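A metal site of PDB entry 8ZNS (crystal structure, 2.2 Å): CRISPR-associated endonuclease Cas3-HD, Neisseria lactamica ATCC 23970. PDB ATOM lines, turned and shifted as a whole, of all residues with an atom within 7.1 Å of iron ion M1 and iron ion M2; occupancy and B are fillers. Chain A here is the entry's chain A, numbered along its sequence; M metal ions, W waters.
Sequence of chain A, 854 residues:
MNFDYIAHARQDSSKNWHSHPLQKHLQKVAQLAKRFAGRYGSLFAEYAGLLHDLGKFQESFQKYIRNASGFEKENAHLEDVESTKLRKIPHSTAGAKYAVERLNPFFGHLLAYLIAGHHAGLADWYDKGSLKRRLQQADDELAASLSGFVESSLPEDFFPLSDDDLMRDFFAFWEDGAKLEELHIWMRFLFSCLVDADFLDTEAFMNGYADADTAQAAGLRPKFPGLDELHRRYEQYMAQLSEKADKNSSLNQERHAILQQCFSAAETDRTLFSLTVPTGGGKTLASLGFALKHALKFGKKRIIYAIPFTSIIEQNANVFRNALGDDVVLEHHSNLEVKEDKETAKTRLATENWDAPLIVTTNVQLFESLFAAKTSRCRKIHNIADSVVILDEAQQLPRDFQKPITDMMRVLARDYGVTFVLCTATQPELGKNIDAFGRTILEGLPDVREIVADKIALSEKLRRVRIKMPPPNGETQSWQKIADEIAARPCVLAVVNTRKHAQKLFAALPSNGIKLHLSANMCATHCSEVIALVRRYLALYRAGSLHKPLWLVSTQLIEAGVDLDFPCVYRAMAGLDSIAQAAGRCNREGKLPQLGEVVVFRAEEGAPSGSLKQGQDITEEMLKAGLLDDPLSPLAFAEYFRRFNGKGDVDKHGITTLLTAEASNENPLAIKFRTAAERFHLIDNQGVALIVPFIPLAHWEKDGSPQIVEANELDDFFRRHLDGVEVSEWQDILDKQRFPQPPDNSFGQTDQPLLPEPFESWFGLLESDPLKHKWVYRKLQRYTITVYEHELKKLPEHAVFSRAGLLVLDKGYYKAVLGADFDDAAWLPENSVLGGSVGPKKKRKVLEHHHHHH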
ATOM      1  N   ALA A   7     -22.161   3.648 -22.936  1.00  0.00           N
ATOM      2  CA  ALA A   7     -22.647   4.611 -21.953  1.00  0.00           C
ATOM      3  C   ALA A   7     -23.774   5.484 -22.470  1.00  0.00           C
ATOM      4  O   ALA A   7     -24.637   5.870 -21.692  1.00  0.00           O
ATOM      5  CB  ALA A   7     -21.501   5.518 -21.478  1.00  0.00           C
ATOM      6  N   HIS A   8     -23.775   5.787 -23.769  1.00  0.00           N
ATOM      7  CA  HIS A   8     -24.772   6.644 -24.395  1.00  0.00           C
ATOM      8  C   HIS A   8     -24.990   6.207 -25.843  1.00  0.00           C
ATOM      9  O   HIS A   8     -24.119   5.584 -26.463  1.00  0.00           O
ATOM     10  CB  HIS A   8     -24.365   8.142 -24.412  1.00  0.00           C
ATOM     11  CG  HIS A   8     -23.840   8.655 -23.103  1.00  0.00           C
ATOM     12  ND1 HIS A   8     -22.491   8.714 -22.815  1.00  0.00           N
ATOM     13  CD2 HIS A   8     -24.478   9.159 -22.017  1.00  0.00           C
ATOM     14  CE1 HIS A   8     -22.326   9.217 -21.602  1.00  0.00           C
ATOM     15  NE2 HIS A   8     -23.518   9.487 -21.100  1.00  0.00           N
ATOM     16  N   HIS A  20     -21.337   5.515 -27.438  1.00  0.00           N
ATOM     17  CA  HIS A  20     -20.210   5.967 -26.629  1.00  0.00           C
ATOM     18  C   HIS A  20     -19.669   4.805 -25.807  1.00  0.00           C
ATOM     19  O   HIS A  20     -20.389   4.299 -24.940  1.00  0.00           O
ATOM     20  CB  HIS A  20     -20.692   7.100 -25.728  1.00  0.00           C
ATOM     21  CG  HIS A  20     -19.621   7.962 -25.147  1.00  0.00           C
ATOM     22  ND1 HIS A  20     -19.870   8.839 -24.119  1.00  0.00           N
ATOM     23  CD2 HIS A  20     -18.301   8.088 -25.441  1.00  0.00           C
ATOM     24  CE1 HIS A  20     -18.753   9.480 -23.804  1.00  0.00           C
ATOM     25  NE2 HIS A  20     -17.790   9.032 -24.580  1.00  0.00           N
ATOM     26  N   LEU A  22     -18.349   2.469 -22.988  1.00  0.00           N
ATOM     27  CA  LEU A  22     -18.458   2.702 -21.549  1.00  0.00           C
ATOM     28  C   LEU A  22     -17.081   2.788 -20.885  1.00  0.00           C
ATOM     29  O   LEU A  22     -16.827   3.693 -20.079  1.00  0.00           O
ATOM     30  CB  LEU A  22     -19.313   1.598 -20.902  1.00  0.00           C
ATOM     31  CG  LEU A  22     -19.469   1.574 -19.365  1.00  0.00           C
ATOM     32  CD1 LEU A  22     -20.000   2.931 -18.804  1.00  0.00           C
ATOM     33  CD2 LEU A  22     -20.350   0.416 -18.898  1.00  0.00           C
ATOM     34  N   HIS A  25     -15.405   6.122 -21.560  1.00  0.00           N
ATOM     35  CA  HIS A  25     -16.063   7.231 -20.886  1.00  0.00           C
ATOM     36  C   HIS A  25     -15.712   7.235 -19.397  1.00  0.00           C
ATOM     37  O   HIS A  25     -15.423   8.306 -18.838  1.00  0.00           O
ATOM     38  CB  HIS A  25     -17.573   7.113 -21.126  1.00  0.00           C
ATOM     39  CG  HIS A  25     -18.414   8.024 -20.287  1.00  0.00           C
ATOM     40  ND1 HIS A  25     -18.556   9.368 -20.541  1.00  0.00           N
ATOM     41  CD2 HIS A  25     -19.191   7.755 -19.207  1.00  0.00           C
ATOM     42  CE1 HIS A  25     -19.368   9.895 -19.645  1.00  0.00           C
ATOM     43  NE2 HIS A  25     -19.766   8.942 -18.831  1.00  0.00           N
ATOM     44  N   LEU A  26     -15.693   6.057 -18.754  1.00  0.00           N
ATOM     45  CA  LEU A  26     -15.309   6.004 -17.352  1.00  0.00           C
ATOM     46  C   LEU A  26     -13.880   6.487 -17.164  1.00  0.00           C
ATOM     47  O   LEU A  26     -13.581   7.228 -16.210  1.00  0.00           O
ATOM     48  CB  LEU A  26     -15.492   4.589 -16.784  1.00  0.00           C
ATOM     49  CG  LEU A  26     -16.919   4.061 -16.591  1.00  0.00           C
ATOM     50  CD1 LEU A  26     -16.879   2.577 -16.121  1.00  0.00           C
ATOM     51  CD2 LEU A  26     -17.696   4.916 -15.623  1.00  0.00           C
ATOM     52  N   VAL A  29     -13.780  10.407 -17.890  1.00  0.00           N
ATOM     53  CA  VAL A  29     -14.444  11.194 -16.862  1.00  0.00           C
ATOM     54  C   VAL A  29     -13.625  11.175 -15.581  1.00  0.00           C
ATOM     55  O   VAL A  29     -13.482  12.214 -14.931  1.00  0.00           O
ATOM     56  CB  VAL A  29     -15.884  10.689 -16.644  1.00  0.00           C
ATOM     57  CG1 VAL A  29     -16.490  11.256 -15.359  1.00  0.00           C
ATOM     58  CG2 VAL A  29     -16.723  11.082 -17.848  1.00  0.00           C
ATOM     59  N   GLY A  49     -15.312   9.729 -10.706  1.00  0.00           N
ATOM     60  CA  GLY A  49     -15.494   9.646 -12.156  1.00  0.00           C
ATOM     61  C   GLY A  49     -15.427   8.210 -12.648  1.00  0.00           C
ATOM     62  O   GLY A  49     -16.193   7.810 -13.544  1.00  0.00           O
ATOM     63  N   HIS A  52     -18.824   6.423 -11.380  1.00  0.00           N
ATOM     64  CA  HIS A  52     -20.151   7.035 -11.479  1.00  0.00           C
ATOM     65  C   HIS A  52     -21.095   6.205 -12.359  1.00  0.00           C
ATOM     66  O   HIS A  52     -22.241   5.957 -11.967  1.00  0.00           O
ATOM     67  CB  HIS A  52     -20.026   8.496 -11.970  1.00  0.00           C
ATOM     68  CG  HIS A  52     -19.945   8.655 -13.462  1.00  0.00           C
ATOM     69  ND1 HIS A  52     -18.808   8.344 -14.189  1.00  0.00           N
ATOM     70  CD2 HIS A  52     -20.851   9.114 -14.366  1.00  0.00           C
ATOM     71  CE1 HIS A  52     -19.032   8.594 -15.462  1.00  0.00           C
ATOM     72  NE2 HIS A  52     -20.263   9.044 -15.610  1.00  0.00           N
ATOM     73  N   ASP A  53     -20.608   5.701 -13.502  1.00  0.00           N
ATOM     74  CA  ASP A  53     -21.454   4.914 -14.404  1.00  0.00           C
ATOM     75  C   ASP A  53     -21.208   3.406 -14.286  1.00  0.00           C
ATOM     76  O   ASP A  53     -21.444   2.655 -15.247  1.00  0.00           O
ATOM     77  CB  ASP A  53     -21.281   5.370 -15.872  1.00  0.00           C
ATOM     78  CG  ASP A  53     -22.081   6.646 -16.220  1.00  0.00           C
ATOM     79  OD1 ASP A  53     -22.984   7.076 -15.457  1.00  0.00           O
ATOM     80  OD2 ASP A  53     -21.786   7.237 -17.282  1.00  0.00           O
ATOM     81  N   LYS A  56     -23.996   1.018 -15.443  1.00  0.00           N
ATOM     82  CA  LYS A  56     -24.382   0.725 -16.810  1.00  0.00           C
ATOM     83  C   LYS A  56     -23.830  -0.620 -17.290  1.00  0.00           C
ATOM     84  O   LYS A  56     -24.213  -1.070 -18.365  1.00  0.00           O
ATOM     85  CB  LYS A  56     -23.944   1.854 -17.745  1.00  0.00           C
ATOM     86  CG  LYS A  56     -24.705   3.146 -17.529  1.00  0.00           C
ATOM     87  CD  LYS A  56     -24.087   4.297 -18.361  1.00  0.00           C
ATOM     88  CE  LYS A  56     -24.939   5.568 -18.244  1.00  0.00           C
ATOM     89  NZ  LYS A  56     -24.225   6.803 -18.713  1.00  0.00           N
ATOM     90  N   HIS A  77     -29.934   6.993 -20.312  1.00  0.00           N
ATOM     91  CA  HIS A  77     -29.127   7.260 -19.134  1.00  0.00           C
ATOM     92  C   HIS A  77     -29.801   8.239 -18.165  1.00  0.00           C
ATOM     93  O   HIS A  77     -29.295   8.411 -17.054  1.00  0.00           O
ATOM     94  CB  HIS A  77     -27.769   7.803 -19.556  1.00  0.00           C
ATOM     95  CG  HIS A  77     -27.847   8.983 -20.484  1.00  0.00           C
ATOM     96  ND1 HIS A  77     -28.495   8.927 -21.696  1.00  0.00           N
ATOM     97  CD2 HIS A  77     -27.375  10.245 -20.365  1.00  0.00           C
ATOM     98  CE1 HIS A  77     -28.420  10.113 -22.293  1.00  0.00           C
ATOM     99  NE2 HIS A  77     -27.748  10.920 -21.503  1.00  0.00           N
ATOM    100  N   LEU A  78     -30.899   8.887 -18.550  1.00  0.00           N
ATOM    101  CA  LEU A  78     -31.569   9.843 -17.655  1.00  0.00           C
ATOM    102  C   LEU A  78     -32.494   9.092 -16.707  1.00  0.00           C
ATOM    103  O   LEU A  78     -33.708   9.005 -16.929  1.00  0.00           O
ATOM    104  CB  LEU A  78     -32.339  10.892 -18.469  1.00  0.00           C
ATOM    105  CG  LEU A  78     -31.517  12.032 -19.087  1.00  0.00           C
ATOM    106  CD1 LEU A  78     -30.596  11.499 -20.171  1.00  0.00           C
ATOM    107  CD2 LEU A  78     -32.415  13.121 -19.651  1.00  0.00           C
ATOM    108  N   GLU A  79     -31.923   8.576 -15.595  1.00  0.00           N
ATOM    109  CA  GLU A  79     -32.684   7.780 -14.619  1.00  0.00           C
ATOM    110  C   GLU A  79     -33.823   8.555 -13.951  1.00  0.00           C
ATOM    111  O   GLU A  79     -34.778   7.929 -13.472  1.00  0.00           O
ATOM    112  CB  GLU A  79     -31.756   7.180 -13.540  1.00  0.00           C
ATOM    113  CG  GLU A  79     -30.441   7.984 -13.221  1.00  0.00           C
ATOM    114  CD  GLU A  79     -29.556   7.354 -12.120  1.00  0.00           C
ATOM    115  OE1 GLU A  79     -29.231   8.052 -11.131  1.00  0.00           O
ATOM    116  OE2 GLU A  79     -29.176   6.182 -12.223  1.00  0.00           O
ATOM    117  N   HIS A  91     -28.908   3.339 -12.673  1.00  0.00           N
ATOM    118  CA  HIS A  91     -27.504   2.981 -12.783  1.00  0.00           C
ATOM    119  C   HIS A  91     -26.569   3.752 -11.851  1.00  0.00           C
ATOM    120  O   HIS A  91     -25.436   3.313 -11.651  1.00  0.00           O
ATOM    121  CB  HIS A  91     -27.033   3.174 -14.239  1.00  0.00           C
ATOM    122  CG  HIS A  91     -26.891   4.613 -14.634  1.00  0.00           C
ATOM    123  ND1 HIS A  91     -27.928   5.339 -15.185  1.00  0.00           N
ATOM    124  CD2 HIS A  91     -25.848   5.466 -14.509  1.00  0.00           C
ATOM    125  CE1 HIS A  91     -27.521   6.576 -15.397  1.00  0.00           C
ATOM    126  NE2 HIS A  91     -26.255   6.674 -15.014  1.00  0.00           N
ATOM    127  N   SER A  92     -27.011   4.860 -11.230  1.00  0.00           N
ATOM    128  CA  SER A  92     -26.068   5.683 -10.463  1.00  0.00           C
ATOM    129  C   SER A  92     -25.704   5.069  -9.124  1.00  0.00           C
ATOM    130  O   SER A  92     -24.655   5.402  -8.580  1.00  0.00           O
ATOM    131  CB  SER A  92     -26.628   7.092 -10.213  1.00  0.00           C
ATOM    132  OG  SER A  92     -27.880   7.102  -9.515  1.00  0.00           O
ATOM    133  N   ILE A 115     -21.593   9.988  -6.251  1.00  0.00           N
ATOM    134  CA  ILE A 115     -21.910   9.050  -7.327  1.00  0.00           C
ATOM    135  C   ILE A 115     -23.413   8.902  -7.472  1.00  0.00           C
ATOM    136  O   ILE A 115     -23.948   8.898  -8.583  1.00  0.00           O
ATOM    137  CB  ILE A 115     -21.254   7.683  -7.084  1.00  0.00           C
ATOM    138  CG1 ILE A 115     -19.745   7.756  -7.205  1.00  0.00           C
ATOM    139  CG2 ILE A 115     -21.799   6.653  -8.094  1.00  0.00           C
ATOM    140  CD1 ILE A 115     -19.117   6.552  -6.548  1.00  0.00           C
ATOM    141  N   HIS A 118     -25.299  11.954  -9.160  1.00  0.00           N
ATOM    142  CA  HIS A 118     -24.808  12.532 -10.410  1.00  0.00           C
ATOM    143  C   HIS A 118     -25.919  12.704 -11.456  1.00  0.00           C
ATOM    144  O   HIS A 118     -25.717  13.424 -12.441  1.00  0.00           O
ATOM    145  CB  HIS A 118     -23.613  11.722 -10.941  1.00  0.00           C
ATOM    146  CG  HIS A 118     -23.948  10.568 -11.844  1.00  0.00           C
ATOM    147  ND1 HIS A 118     -23.923   9.257 -11.419  1.00  0.00           N
ATOM    148  CD2 HIS A 118     -24.223  10.520 -13.172  1.00  0.00           C
ATOM    149  CE1 HIS A 118     -24.196   8.447 -12.425  1.00  0.00           C
ATOM    150  NE2 HIS A 118     -24.398   9.188 -13.502  1.00  0.00           N
ATOM    151  N   HIS A 119     -27.110  12.143 -11.242  1.00  0.00           N
ATOM    152  CA  HIS A 119     -28.292  12.583 -11.975  1.00  0.00           C
ATOM    153  C   HIS A 119     -29.282  13.367 -11.120  1.00  0.00           C
ATOM    154  O   HIS A 119     -29.686  14.470 -11.494  1.00  0.00           O
ATOM    155  CB  HIS A 119     -29.004  11.368 -12.614  1.00  0.00           C
ATOM    156  CG  HIS A 119     -28.234  10.719 -13.713  1.00  0.00           C
ATOM    157  ND1 HIS A 119     -28.316  11.143 -15.015  1.00  0.00           N
ATOM    158  CD2 HIS A 119     -27.353   9.688 -13.703  1.00  0.00           C
ATOM    159  CE1 HIS A 119     -27.524  10.395 -15.768  1.00  0.00           C
ATOM    160  NE2 HIS A 119     -26.939   9.503 -14.992  1.00  0.00           N
ATOM    161  N   LEU A 194     -16.937  16.193 -10.891  1.00  0.00           N
ATOM    162  CA  LEU A 194     -17.528  15.009 -11.491  1.00  0.00           C
ATOM    163  C   LEU A 194     -18.500  15.401 -12.597  1.00  0.00           C
ATOM    164  O   LEU A 194     -18.389  14.919 -13.735  1.00  0.00           O
ATOM    165  CB  LEU A 194     -18.229  14.194 -10.421  1.00  0.00           C
ATOM    166  CG  LEU A 194     -19.127  13.109 -10.971  1.00  0.00           C
ATOM    167  CD1 LEU A 194     -18.252  12.143 -11.813  1.00  0.00           C
ATOM    168  CD2 LEU A 194     -19.836  12.359  -9.831  1.00  0.00           C
ATOM    169  N   ASP A 198     -18.129  14.743 -16.614  1.00  0.00           N
ATOM    170  CA  ASP A 198     -19.110  13.837 -17.215  1.00  0.00           C
ATOM    171  C   ASP A 198     -19.783  14.505 -18.404  1.00  0.00           C
ATOM    172  O   ASP A 198     -19.769  13.980 -19.521  1.00  0.00           O
ATOM    173  CB  ASP A 198     -20.127  13.459 -16.131  1.00  0.00           C
ATOM    174  CG  ASP A 198     -21.080  12.338 -16.524  1.00  0.00           C
ATOM    175  OD1 ASP A 198     -20.772  11.460 -17.375  1.00  0.00           O
ATOM    176  OD2 ASP A 198     -22.170  12.295 -15.910  1.00  0.00           O
ATOM    177  N   PHE A 199     -20.349  15.689 -18.169  1.00  0.00           N
ATOM    178  CA  PHE A 199     -21.060  16.412 -19.230  1.00  0.00           C
ATOM    179  C   PHE A 199     -20.132  16.759 -20.382  1.00  0.00           C
ATOM    180  O   PHE A 199     -20.512  16.634 -21.549  1.00  0.00           O
ATOM    181  CB  PHE A 199     -21.704  17.695 -18.666  1.00  0.00           C
ATOM    182  CG  PHE A 199     -22.880  17.445 -17.749  1.00  0.00           C
ATOM    183  CD1 PHE A 199     -23.210  16.146 -17.349  1.00  0.00           C
ATOM    184  CD2 PHE A 199     -23.652  18.495 -17.289  1.00  0.00           C
ATOM    185  CE1 PHE A 199     -24.289  15.896 -16.515  1.00  0.00           C
ATOM    186  CE2 PHE A 199     -24.736  18.264 -16.464  1.00  0.00           C
ATOM    187  CZ  PHE A 199     -25.057  16.943 -16.072  1.00  0.00           C
ATOM    188  N   ASP A 201     -17.365  15.259 -21.403  1.00  0.00           N
ATOM    189  CA  ASP A 201     -17.059  14.060 -22.187  1.00  0.00           C
ATOM    190  C   ASP A 201     -18.242  13.645 -23.050  1.00  0.00           C
ATOM    191  O   ASP A 201     -18.093  13.304 -24.241  1.00  0.00           O
ATOM    192  CB  ASP A 201     -16.669  12.903 -21.254  1.00  0.00           C
ATOM    193  CG  ASP A 201     -16.039  11.732 -22.006  1.00  0.00           C
ATOM    194  OD1 ASP A 201     -14.941  11.927 -22.555  1.00  0.00           O
ATOM    195  OD2 ASP A 201     -16.650  10.645 -22.046  1.00  0.00           O
ATOM    196  N   THR A 202     -19.442  13.660 -22.464  1.00  0.00           N
ATOM    197  CA  THR A 202     -20.616  13.285 -23.245  1.00  0.00           C
ATOM    198  C   THR A 202     -20.837  14.259 -24.398  1.00  0.00           C
ATOM    199  O   THR A 202     -21.239  13.863 -25.490  1.00  0.00           O
ATOM    200  CB  THR A 202     -21.854  13.220 -22.356  1.00  0.00           C
ATOM    201  OG1 THR A 202     -21.546  12.440 -21.206  1.00  0.00           O
ATOM    202  CG2 THR A 202     -23.010  12.565 -23.098  1.00  0.00           C
ATOM    203  N   ARG A 348     -29.886  18.605 -20.851  1.00  0.00           N
ATOM    204  CA  ARG A 348     -29.006  18.329 -19.720  1.00  0.00           C
ATOM    205  C   ARG A 348     -27.597  18.861 -19.985  1.00  0.00           C
ATOM    206  O   ARG A 348     -26.982  19.461 -19.093  1.00  0.00           O
ATOM    207  CB  ARG A 348     -28.962  16.823 -19.433  1.00  0.00           C
ATOM    208  CG  ARG A 348     -28.352  16.417 -18.101  1.00  0.00           C
ATOM    209  CD  ARG A 348     -28.787  15.003 -17.680  1.00  0.00           C
ATOM    210  NE  ARG A 348     -27.959  14.465 -16.603  1.00  0.00           N
ATOM    211  CZ  ARG A 348     -26.877  13.728 -16.811  1.00  0.00           C
ATOM    212  NH1 ARG A 348     -26.469  13.456 -18.045  1.00  0.00           N
ATOM    213  NH2 ARG A 348     -26.188  13.264 -15.776  1.00  0.00           N
HETATM  214 FE    FE M   1     -25.099   8.390 -15.233  1.00  0.00          FE
HETATM  215 FE    FE M   2     -21.357   9.417 -17.463  1.00  0.00          FE
HETATM  216  O   HOH W   1     -24.057  10.067 -17.572  1.00  0.00           O
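Iron ion M1 is bound by NE2 of His 118 (2.0 Å), NE2 of His 91 (2.1 Å), NE2 of His 119 (2.2 Å) and OD1 of Asp 53 (2.5 Å).
Iron ion M1 has four donor atoms within binding distance.
Water W1 bridges the side-chain carboxylate of Asp 198 (3.4 Å) and the side-chain amino group of Lys 56 (3.5 Å).
A ring nitrogen (ND1) of His 118 lies within hydrogen-bond range of the backbone carbonyl oxygen (O) of Ile 115 (2.9 Å).
A ring nitrogen (NE2) of His 119 sits close to the backbone carbonyl oxygen (O) of His 77 (3.3 Å).
NZ of Lys 56 sits close to OD2 of Asp 53.
N of His 91 sits at hydrogen-bond distance from OE2 of Glu 79 (2.9 Å).
ND1 of His 119 is in hydrogen-bond range of NH2 of Arg 348 (3.1 Å).
The guanidinium group of Arg 348 is in hydrogen-bond range of the backbone carbonyl oxygen of His 118, at 3.4 Å.
The side-chain carboxylate of Asp 201 is in hydrogen-bond range of a ring nitrogen (ND1) of His 25, at 2.7 Å.
The side-chain amino group (NZ) of Lys 56 is in hydrogen-bond range of the backbone carbonyl oxygen (O) of Ala 7.
Within 4 Å of iron ion M2: His 25, His 52, Asp 53 and Asp 198.
The nearest printed residue that does not touch iron ion M2 is Lys 56 (4.1 Å).
Merely in contact with iron ion M1: Lys 56 (3.9 Å).
Within 4 Å of iron ion M1: Asp 53, Lys 56, His 91, His 118 and His 119.
The side-chain carboxylate (OD1) of Asp 198 binds iron ion M2.
Iron ion M2 is bound by NE2 of His 25, 2.2 Å away.
NE2 of His 52 is bound to iron ion M2 (2.2 Å).
OD2 of Asp 53 binds iron ion M2, 2.2 Å away.
Slightly farther from iron ion M2 lies water W1 (2.8 Å).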
